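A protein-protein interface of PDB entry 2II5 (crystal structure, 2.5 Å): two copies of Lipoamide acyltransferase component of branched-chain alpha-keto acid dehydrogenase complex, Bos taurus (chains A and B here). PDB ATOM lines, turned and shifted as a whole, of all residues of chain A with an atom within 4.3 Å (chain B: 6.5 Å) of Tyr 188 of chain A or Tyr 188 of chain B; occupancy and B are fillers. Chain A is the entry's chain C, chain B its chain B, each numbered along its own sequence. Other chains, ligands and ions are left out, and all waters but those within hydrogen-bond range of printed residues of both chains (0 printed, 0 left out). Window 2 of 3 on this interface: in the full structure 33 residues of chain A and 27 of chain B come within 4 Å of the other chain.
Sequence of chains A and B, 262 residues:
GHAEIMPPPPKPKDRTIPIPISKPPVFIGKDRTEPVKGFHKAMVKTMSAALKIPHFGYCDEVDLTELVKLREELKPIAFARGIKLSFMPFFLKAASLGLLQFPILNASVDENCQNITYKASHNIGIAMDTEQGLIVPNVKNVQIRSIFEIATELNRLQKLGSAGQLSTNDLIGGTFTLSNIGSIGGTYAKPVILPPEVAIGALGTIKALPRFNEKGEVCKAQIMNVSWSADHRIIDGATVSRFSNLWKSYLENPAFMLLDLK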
ATOM      1  N   TYR A  58       8.946 -30.298   9.962  1.00  0.00           N
ATOM      2  CA  TYR A  58       8.655 -28.947   9.554  1.00  0.00           C
ATOM      3  C   TYR A  58       7.305 -28.495  10.149  1.00  0.00           C
ATOM      4  O   TYR A  58       6.289 -29.179  10.011  1.00  0.00           O
ATOM      5  CB  TYR A  58       8.642 -28.855   8.024  1.00  0.00           C
ATOM      6  CG  TYR A  58       8.031 -27.581   7.461  1.00  0.00           C
ATOM      7  CD1 TYR A  58       6.654 -27.448   7.334  1.00  0.00           C
ATOM      8  CD2 TYR A  58       8.821 -26.524   7.041  1.00  0.00           C
ATOM      9  CE1 TYR A  58       6.064 -26.265   6.819  1.00  0.00           C
ATOM     10  CE2 TYR A  58       8.257 -25.327   6.517  1.00  0.00           C
ATOM     11  CZ  TYR A  58       6.869 -25.226   6.424  1.00  0.00           C
ATOM     12  OH  TYR A  58       6.261 -24.107   5.898  1.00  0.00           O
ATOM     13  N   CYS A  59       7.282 -27.316  10.753  1.00  0.00           N
ATOM     14  CA  CYS A  59       6.079 -26.888  11.431  1.00  0.00           C
ATOM     15  C   CYS A  59       5.559 -25.561  10.956  1.00  0.00           C
ATOM     16  O   CYS A  59       6.280 -24.804  10.302  1.00  0.00           O
ATOM     17  CB  CYS A  59       6.313 -26.818  12.939  1.00  0.00           C
ATOM     18  SG  CYS A  59       6.929 -28.360  13.521  1.00  0.00           S
ATOM     19  N   ASP A  60       4.300 -25.273  11.305  1.00  0.00           N
ATOM     20  CA  ASP A  60       3.694 -23.996  10.966  1.00  0.00           C
ATOM     21  C   ASP A  60       2.501 -23.666  11.862  1.00  0.00           C
ATOM     22  O   ASP A  60       2.049 -24.504  12.651  1.00  0.00           O
ATOM     23  CB  ASP A  60       3.329 -23.945   9.480  1.00  0.00           C
ATOM     24  CG  ASP A  60       3.427 -22.506   8.884  1.00  0.00           C
ATOM     25  OD1 ASP A  60       3.544 -21.517   9.651  1.00  0.00           O
ATOM     26  OD2 ASP A  60       3.405 -22.368   7.635  1.00  0.00           O
ATOM     27  N   THR A 187       0.359 -28.188  21.113  1.00  0.00           N
ATOM     28  CA  THR A 187       0.633 -27.195  20.073  1.00  0.00           C
ATOM     29  C   THR A 187       1.410 -27.928  18.967  1.00  0.00           C
ATOM     30  O   THR A 187       0.795 -28.504  18.055  1.00  0.00           O
ATOM     31  CB  THR A 187       1.458 -26.026  20.628  1.00  0.00           C
ATOM     32  OG1 THR A 187       2.669 -26.532  21.250  1.00  0.00           O
ATOM     33  CG2 THR A 187       0.636 -25.187  21.627  1.00  0.00           C
ATOM     34  N   TYR A 188       2.737 -28.008  19.105  1.00  0.00           N
ATOM     35  CA  TYR A 188       3.625 -28.709  18.157  1.00  0.00           C
ATOM     36  C   TYR A 188       3.937 -30.143  18.583  1.00  0.00           C
ATOM     37  O   TYR A 188       3.804 -30.513  19.759  1.00  0.00           O
ATOM     38  CB  TYR A 188       4.918 -27.951  17.994  1.00  0.00           C
ATOM     39  CG  TYR A 188       4.770 -26.564  17.375  1.00  0.00           C
ATOM     40  CD1 TYR A 188       4.554 -26.428  15.990  1.00  0.00           C
ATOM     41  CD2 TYR A 188       4.871 -25.369  18.152  1.00  0.00           C
ATOM     42  CE1 TYR A 188       4.409 -25.166  15.396  1.00  0.00           C
ATOM     43  CE2 TYR A 188       4.733 -24.089  17.536  1.00  0.00           C
ATOM     44  CZ  TYR A 188       4.511 -24.010  16.150  1.00  0.00           C
ATOM     45  OH  TYR A 188       4.445 -22.805  15.427  1.00  0.00           O
ATOM     46  N   ALA A 189       4.335 -30.970  17.623  1.00  0.00           N
ATOM     47  CA  ALA A 189       4.655 -32.349  17.942  1.00  0.00           C
ATOM     48  C   ALA A 189       5.759 -32.887  17.056  1.00  0.00           C
ATOM     49  O   ALA A 189       6.159 -32.248  16.122  1.00  0.00           O
ATOM     50  CB  ALA A 189       3.412 -33.205  17.844  1.00  0.00           C
ATOM     51  N   ASN A 225      -1.623 -25.142  15.518  1.00  0.00           N
ATOM     52  CA  ASN A 225      -0.291 -25.530  15.060  1.00  0.00           C
ATOM     53  C   ASN A 225      -0.302 -26.814  14.231  1.00  0.00           C
ATOM     54  O   ASN A 225      -1.061 -27.726  14.541  1.00  0.00           O
ATOM     55  CB  ASN A 225       0.639 -25.663  16.252  1.00  0.00           C
ATOM     56  CG  ASN A 225       0.853 -24.334  16.950  1.00  0.00           C
ATOM     57  OD1 ASN A 225       0.528 -24.180  18.138  1.00  0.00           O
ATOM     58  ND2 ASN A 225       1.360 -23.345  16.206  1.00  0.00           N
ATOM     59  N   VAL A 226       0.505 -26.873  13.171  1.00  0.00           N
ATOM     60  CA  VAL A 226       0.672 -28.115  12.406  1.00  0.00           C
ATOM     61  C   VAL A 226       2.161 -28.530  12.451  1.00  0.00           C
ATOM     62  O   VAL A 226       3.078 -27.651  12.413  1.00  0.00           O
ATOM     63  CB  VAL A 226       0.136 -27.967  10.958  1.00  0.00           C
ATOM     64  CG1 VAL A 226       0.930 -26.961  10.199  1.00  0.00           C
ATOM     65  CG2 VAL A 226       0.148 -29.283  10.251  1.00  0.00           C
ATOM     66  N   SER A 227       2.392 -29.836  12.597  1.00  0.00           N
ATOM     67  CA  SER A 227       3.747 -30.405  12.648  1.00  0.00           C
ATOM     68  C   SER A 227       3.813 -31.559  11.684  1.00  0.00           C
ATOM     69  O   SER A 227       3.109 -32.533  11.880  1.00  0.00           O
ATOM     70  CB  SER A 227       4.019 -30.968  14.029  1.00  0.00           C
ATOM     71  OG  SER A 227       3.908 -29.974  15.048  1.00  0.00           O
ATOM     72  N   CYS B  59      15.067 -25.080  20.312  1.00  0.00           N
ATOM     73  CA  CYS B  59      14.449 -24.019  19.514  1.00  0.00           C
ATOM     74  C   CYS B  59      14.362 -22.752  20.292  1.00  0.00           C
ATOM     75  O   CYS B  59      14.515 -22.756  21.503  1.00  0.00           O
ATOM     76  CB  CYS B  59      13.081 -24.423  19.048  1.00  0.00           C
ATOM     77  SG  CYS B  59      13.126 -25.942  18.172  1.00  0.00           S
ATOM     78  N   ASP B  60      14.202 -21.642  19.591  1.00  0.00           N
ATOM     79  CA  ASP B  60      13.946 -20.386  20.249  1.00  0.00           C
ATOM     80  C   ASP B  60      13.168 -19.431  19.334  1.00  0.00           C
ATOM     81  O   ASP B  60      12.851 -19.770  18.185  1.00  0.00           O
ATOM     82  CB  ASP B  60      15.259 -19.722  20.735  1.00  0.00           C
ATOM     83  CG  ASP B  60      15.014 -18.778  21.941  1.00  0.00           C
ATOM     84  OD1 ASP B  60      13.807 -18.563  22.232  1.00  0.00           O
ATOM     85  OD2 ASP B  60      15.978 -18.275  22.583  1.00  0.00           O
ATOM     86  N   GLU B  61      12.851 -18.243  19.849  1.00  0.00           N
ATOM     87  CA  GLU B  61      12.313 -17.220  18.987  1.00  0.00           C
ATOM     88  C   GLU B  61      13.250 -16.043  19.115  1.00  0.00           C
ATOM     89  O   GLU B  61      13.845 -15.821  20.179  1.00  0.00           O
ATOM     90  CB  GLU B  61      10.845 -16.869  19.323  1.00  0.00           C
ATOM     91  CG  GLU B  61      10.580 -15.916  20.554  1.00  0.00           C
ATOM     92  CD  GLU B  61       9.111 -15.423  20.570  1.00  0.00           C
ATOM     93  OE1 GLU B  61       8.203 -16.221  20.210  1.00  0.00           O
ATOM     94  OE2 GLU B  61       8.860 -14.231  20.892  1.00  0.00           O
ATOM     95  N   ILE B 181      14.384 -22.351   5.639  1.00  0.00           N
ATOM     96  CA  ILE B 181      13.058 -22.841   5.304  1.00  0.00           C
ATOM     97  C   ILE B 181      12.140 -21.625   5.223  1.00  0.00           C
ATOM     98  O   ILE B 181      11.184 -21.593   4.480  1.00  0.00           O
ATOM     99  CB  ILE B 181      12.534 -23.895   6.345  1.00  0.00           C
ATOM    100  CG1 ILE B 181      12.116 -23.235   7.649  1.00  0.00           C
ATOM    101  CG2 ILE B 181      13.580 -24.949   6.679  1.00  0.00           C
ATOM    102  CD1 ILE B 181      11.906 -24.270   8.808  1.00  0.00           C
ATOM    103  N   GLY B 186       6.833 -21.780   7.398  1.00  0.00           N
ATOM    104  CA  GLY B 186       7.168 -22.530   8.602  1.00  0.00           C
ATOM    105  C   GLY B 186       7.506 -21.675   9.788  1.00  0.00           C
ATOM    106  O   GLY B 186       7.823 -20.471   9.665  1.00  0.00           O
ATOM    107  N   THR B 187       7.477 -22.311  10.956  1.00  0.00           N
ATOM    108  CA  THR B 187       7.885 -21.643  12.161  1.00  0.00           C
ATOM    109  C   THR B 187       9.096 -22.388  12.662  1.00  0.00           C
ATOM    110  O   THR B 187      10.252 -21.956  12.454  1.00  0.00           O
ATOM    111  CB  THR B 187       6.771 -21.662  13.203  1.00  0.00           C
ATOM    112  OG1 THR B 187       6.119 -22.950  13.203  1.00  0.00           O
ATOM    113  CG2 THR B 187       5.738 -20.559  12.872  1.00  0.00           C
ATOM    114  N   TYR B 188       8.816 -23.538  13.272  1.00  0.00           N
ATOM    115  CA  TYR B 188       9.826 -24.392  13.894  1.00  0.00           C
ATOM    116  C   TYR B 188      10.051 -25.574  12.982  1.00  0.00           C
ATOM    117  O   TYR B 188       9.257 -25.837  12.116  1.00  0.00           O
ATOM    118  CB  TYR B 188       9.338 -24.856  15.278  1.00  0.00           C
ATOM    119  CG  TYR B 188       9.366 -23.781  16.369  1.00  0.00           C
ATOM    120  CD1 TYR B 188      10.579 -23.236  16.795  1.00  0.00           C
ATOM    121  CD2 TYR B 188       8.179 -23.323  17.002  1.00  0.00           C
ATOM    122  CE1 TYR B 188      10.635 -22.285  17.796  1.00  0.00           C
ATOM    123  CE2 TYR B 188       8.232 -22.335  18.029  1.00  0.00           C
ATOM    124  CZ  TYR B 188       9.449 -21.831  18.432  1.00  0.00           C
ATOM    125  OH  TYR B 188       9.590 -20.874  19.457  1.00  0.00           O
ATOM    126  N   ALA B 189      11.164 -26.272  13.140  1.00  0.00           N
ATOM    127  CA  ALA B 189      11.436 -27.407  12.238  1.00  0.00           C
ATOM    128  C   ALA B 189      12.317 -28.375  12.967  1.00  0.00           C
ATOM    129  O   ALA B 189      12.825 -28.055  14.018  1.00  0.00           O
ATOM    130  CB  ALA B 189      12.138 -26.912  10.983  1.00  0.00           C
ATOM    131  N   LYS B 190      12.545 -29.533  12.399  1.00  0.00           N
ATOM    132  CA  LYS B 190      13.612 -30.428  12.941  1.00  0.00           C
ATOM    133  C   LYS B 190      14.547 -30.794  11.783  1.00  0.00           C
ATOM    134  O   LYS B 190      14.239 -31.700  11.001  1.00  0.00           O
ATOM    135  CB  LYS B 190      13.044 -31.724  13.557  1.00  0.00           C
ATOM    136  CG  LYS B 190      14.233 -32.723  13.887  1.00  0.00           C
ATOM    137  CD  LYS B 190      14.094 -34.214  13.415  1.00  0.00           C
ATOM    138  CE  LYS B 190      15.490 -34.854  13.431  1.00  0.00           C
ATOM    139  NZ  LYS B 190      15.537 -36.281  12.811  1.00  0.00           N
ATOM    140  N   ALA B 202      17.671 -24.312  11.369  1.00  0.00           N
ATOM    141  CA  ALA B 202      16.643 -23.982  10.384  1.00  0.00           C
ATOM    142  C   ALA B 202      15.990 -22.694  10.849  1.00  0.00           C
ATOM    143  O   ALA B 202      15.642 -22.574  12.013  1.00  0.00           O
ATOM    144  CB  ALA B 202      15.640 -25.112  10.297  1.00  0.00           C
ATOM    145  N   GLY B 204      12.853 -19.952  10.412  1.00  0.00           N
ATOM    146  CA  GLY B 204      11.492 -19.936   9.973  1.00  0.00           C
ATOM    147  C   GLY B 204      11.130 -18.576   9.416  1.00  0.00           C
ATOM    148  O   GLY B 204      11.964 -17.672   9.304  1.00  0.00           O
ATOM    149  N   ASN B 225      11.496 -17.661  14.225  1.00  0.00           N
ATOM    150  CA  ASN B 225      11.960 -18.858  14.933  1.00  0.00           C
ATOM    151  C   ASN B 225      13.229 -19.457  14.338  1.00  0.00           C
ATOM    152  O   ASN B 225      13.420 -19.464  13.109  1.00  0.00           O
ATOM    153  CB  ASN B 225      10.890 -19.929  14.950  1.00  0.00           C
ATOM    154  CG  ASN B 225       9.596 -19.430  15.473  1.00  0.00           C
ATOM    155  OD1 ASN B 225       8.616 -19.308  14.715  1.00  0.00           O
ATOM    156  ND2 ASN B 225       9.557 -19.125  16.759  1.00  0.00           N
ATOM    157  N   VAL B 226      14.073 -19.961  15.219  1.00  0.00           N
ATOM    158  CA  VAL B 226      15.236 -20.745  14.871  1.00  0.00           C
ATOM    159  C   VAL B 226      15.116 -22.165  15.512  1.00  0.00           C
ATOM    160  O   VAL B 226      14.635 -22.315  16.643  1.00  0.00           O
ATOM    161  CB  VAL B 226      16.475 -20.013  15.409  1.00  0.00           C
ATOM    162  CG1 VAL B 226      16.370 -19.906  16.916  1.00  0.00           C
ATOM    163  CG2 VAL B 226      17.773 -20.717  15.007  1.00  0.00           C
ATOM    164  N   SER B 227      15.534 -23.198  14.809  1.00  0.00           N
ATOM    165  CA  SER B 227      15.532 -24.571  15.357  1.00  0.00           C
ATOM    166  C   SER B 227      16.909 -25.206  15.117  1.00  0.00           C
ATOM    167  O   SER B 227      17.324 -25.387  13.964  1.00  0.00           O
ATOM    168  CB  SER B 227      14.485 -25.438  14.675  1.00  0.00           C
ATOM    169  OG  SER B 227      13.160 -24.902  14.805  1.00  0.00           O
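Tyr 58 of chain A touches Tyr 188 of chain B (C to O, 3.8 Å). Gly 186 of chain B touches Cys 59 of chain A (CA to O, 3.0 Å). Thr 187 of chain B touches Asp 60 of chain A. Tyr 188 of chain B touches Tyr 188 of chain A.
Hydrophobic or aromatic side chains of chain B within 4 Å of the printed part of chain A: Tyr 188. Printed residues of chain A that touch a printed residue of chain B: Tyr 58, Cys 59, Asp 60 and Tyr 188. Hydrophobic or aromatic side chains of chain A that line the printed part of chain B: Tyr 58 and Tyr 188. Among the printed residues, 9 pairs touch across the chains.
N of Gly 186 of chain B sits at hydrogen-bond distance from OH of Tyr 58 of chain A (2.8 Å). N of Gly 186 of chain B is in hydrogen-bond range of OD2 of Asp 60 of chain A, at 3.5 Å. O of Cys 59 of chain A lies within hydrogen-bond range of N of Thr 187 of chain B (2.8 Å). The side-chain hydroxyl (OH) of Tyr 188 of chain A is in hydrogen-bond range of the side-chain hydroxyl (OG1) of Thr 187 of chain B, 2.8 Å away. O of Tyr 188 of chain B sits at hydrogen-bond distance from N of Cys 59 of chain A (2.8 Å).
Printed residues of chain B within 4 Å of Tyr 58 of chain A: Gly 186 (2.8 Å) and Tyr 188 (3.8 Å). Of the printed residues of chain B, Asp 60 of chain A touches Gly 186 and Thr 187. Tyr 188 of chain A touches just these residues of chain B: Thr 187 and Tyr 188. Ile 181 of chain B touches none of the printed residues of chain A. Printed residues of chain A within 4 Å of Gly 186 of chain B: Tyr 58 (2.8 Å), Cys 59 (3.0 Å) and Asp 60 (3.5 Å). Of the printed residues of chain A, Thr 187 of chain B touches Cys 59, Asp 60 and Tyr 188. Tyr 188 of chain B touches just these residues of chain A: Tyr 58 (3.8 Å), Cys 59 (2.8 Å) and Tyr 188 (3.6 Å). The nearest printed residue of chain A that does not touch Tyr 188 of chain B is Asp 60 of chain A (5.1 Å).
The side-chain hydroxyl (OH) of Tyr 188 of chain B sits close to the side-chain amide nitrogen (ND2) of Asn 225 of chain B (3.2 Å). The side-chain sulfur of Cys 59 of chain A is in hydrogen-bond range of the side-chain hydroxyl of Ser 227 of chain A. The backbone NH (N) of Val 226 of chain A is in hydrogen-bond range of the backbone carbonyl oxygen (O) of Asp 60 of chain A (2.9 Å). The side-chain hydroxyl (OH) of Tyr 188 of chain A sits close to the side-chain amide nitrogen (ND2) of Asn 225 of chain A.
Cys 59 of chain A touches Tyr 188 of chain B, but with the chains exchanged Tyr 188 of chain A does not touch Cys 59 of chain B (8.3 Å). Asp 60 of chain A touches Thr 187 of chain B, but with the chains exchanged Thr 187 of chain A does not touch Asp 60 of chain B (12.6 Å). Tyr 188 of chain A touches Thr 187 of chain B, but with the chains exchanged Thr 187 of chain A does not touch Tyr 188 of chain B (7.7 Å). Tyr 188 of chain B touches its own counterpart, Tyr 188 of chain A. 8 positions are printed for both chains. Of the 9 pairs that touch across the chains among the printed residues, 1 has its exchanged pair printed and touching as well.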
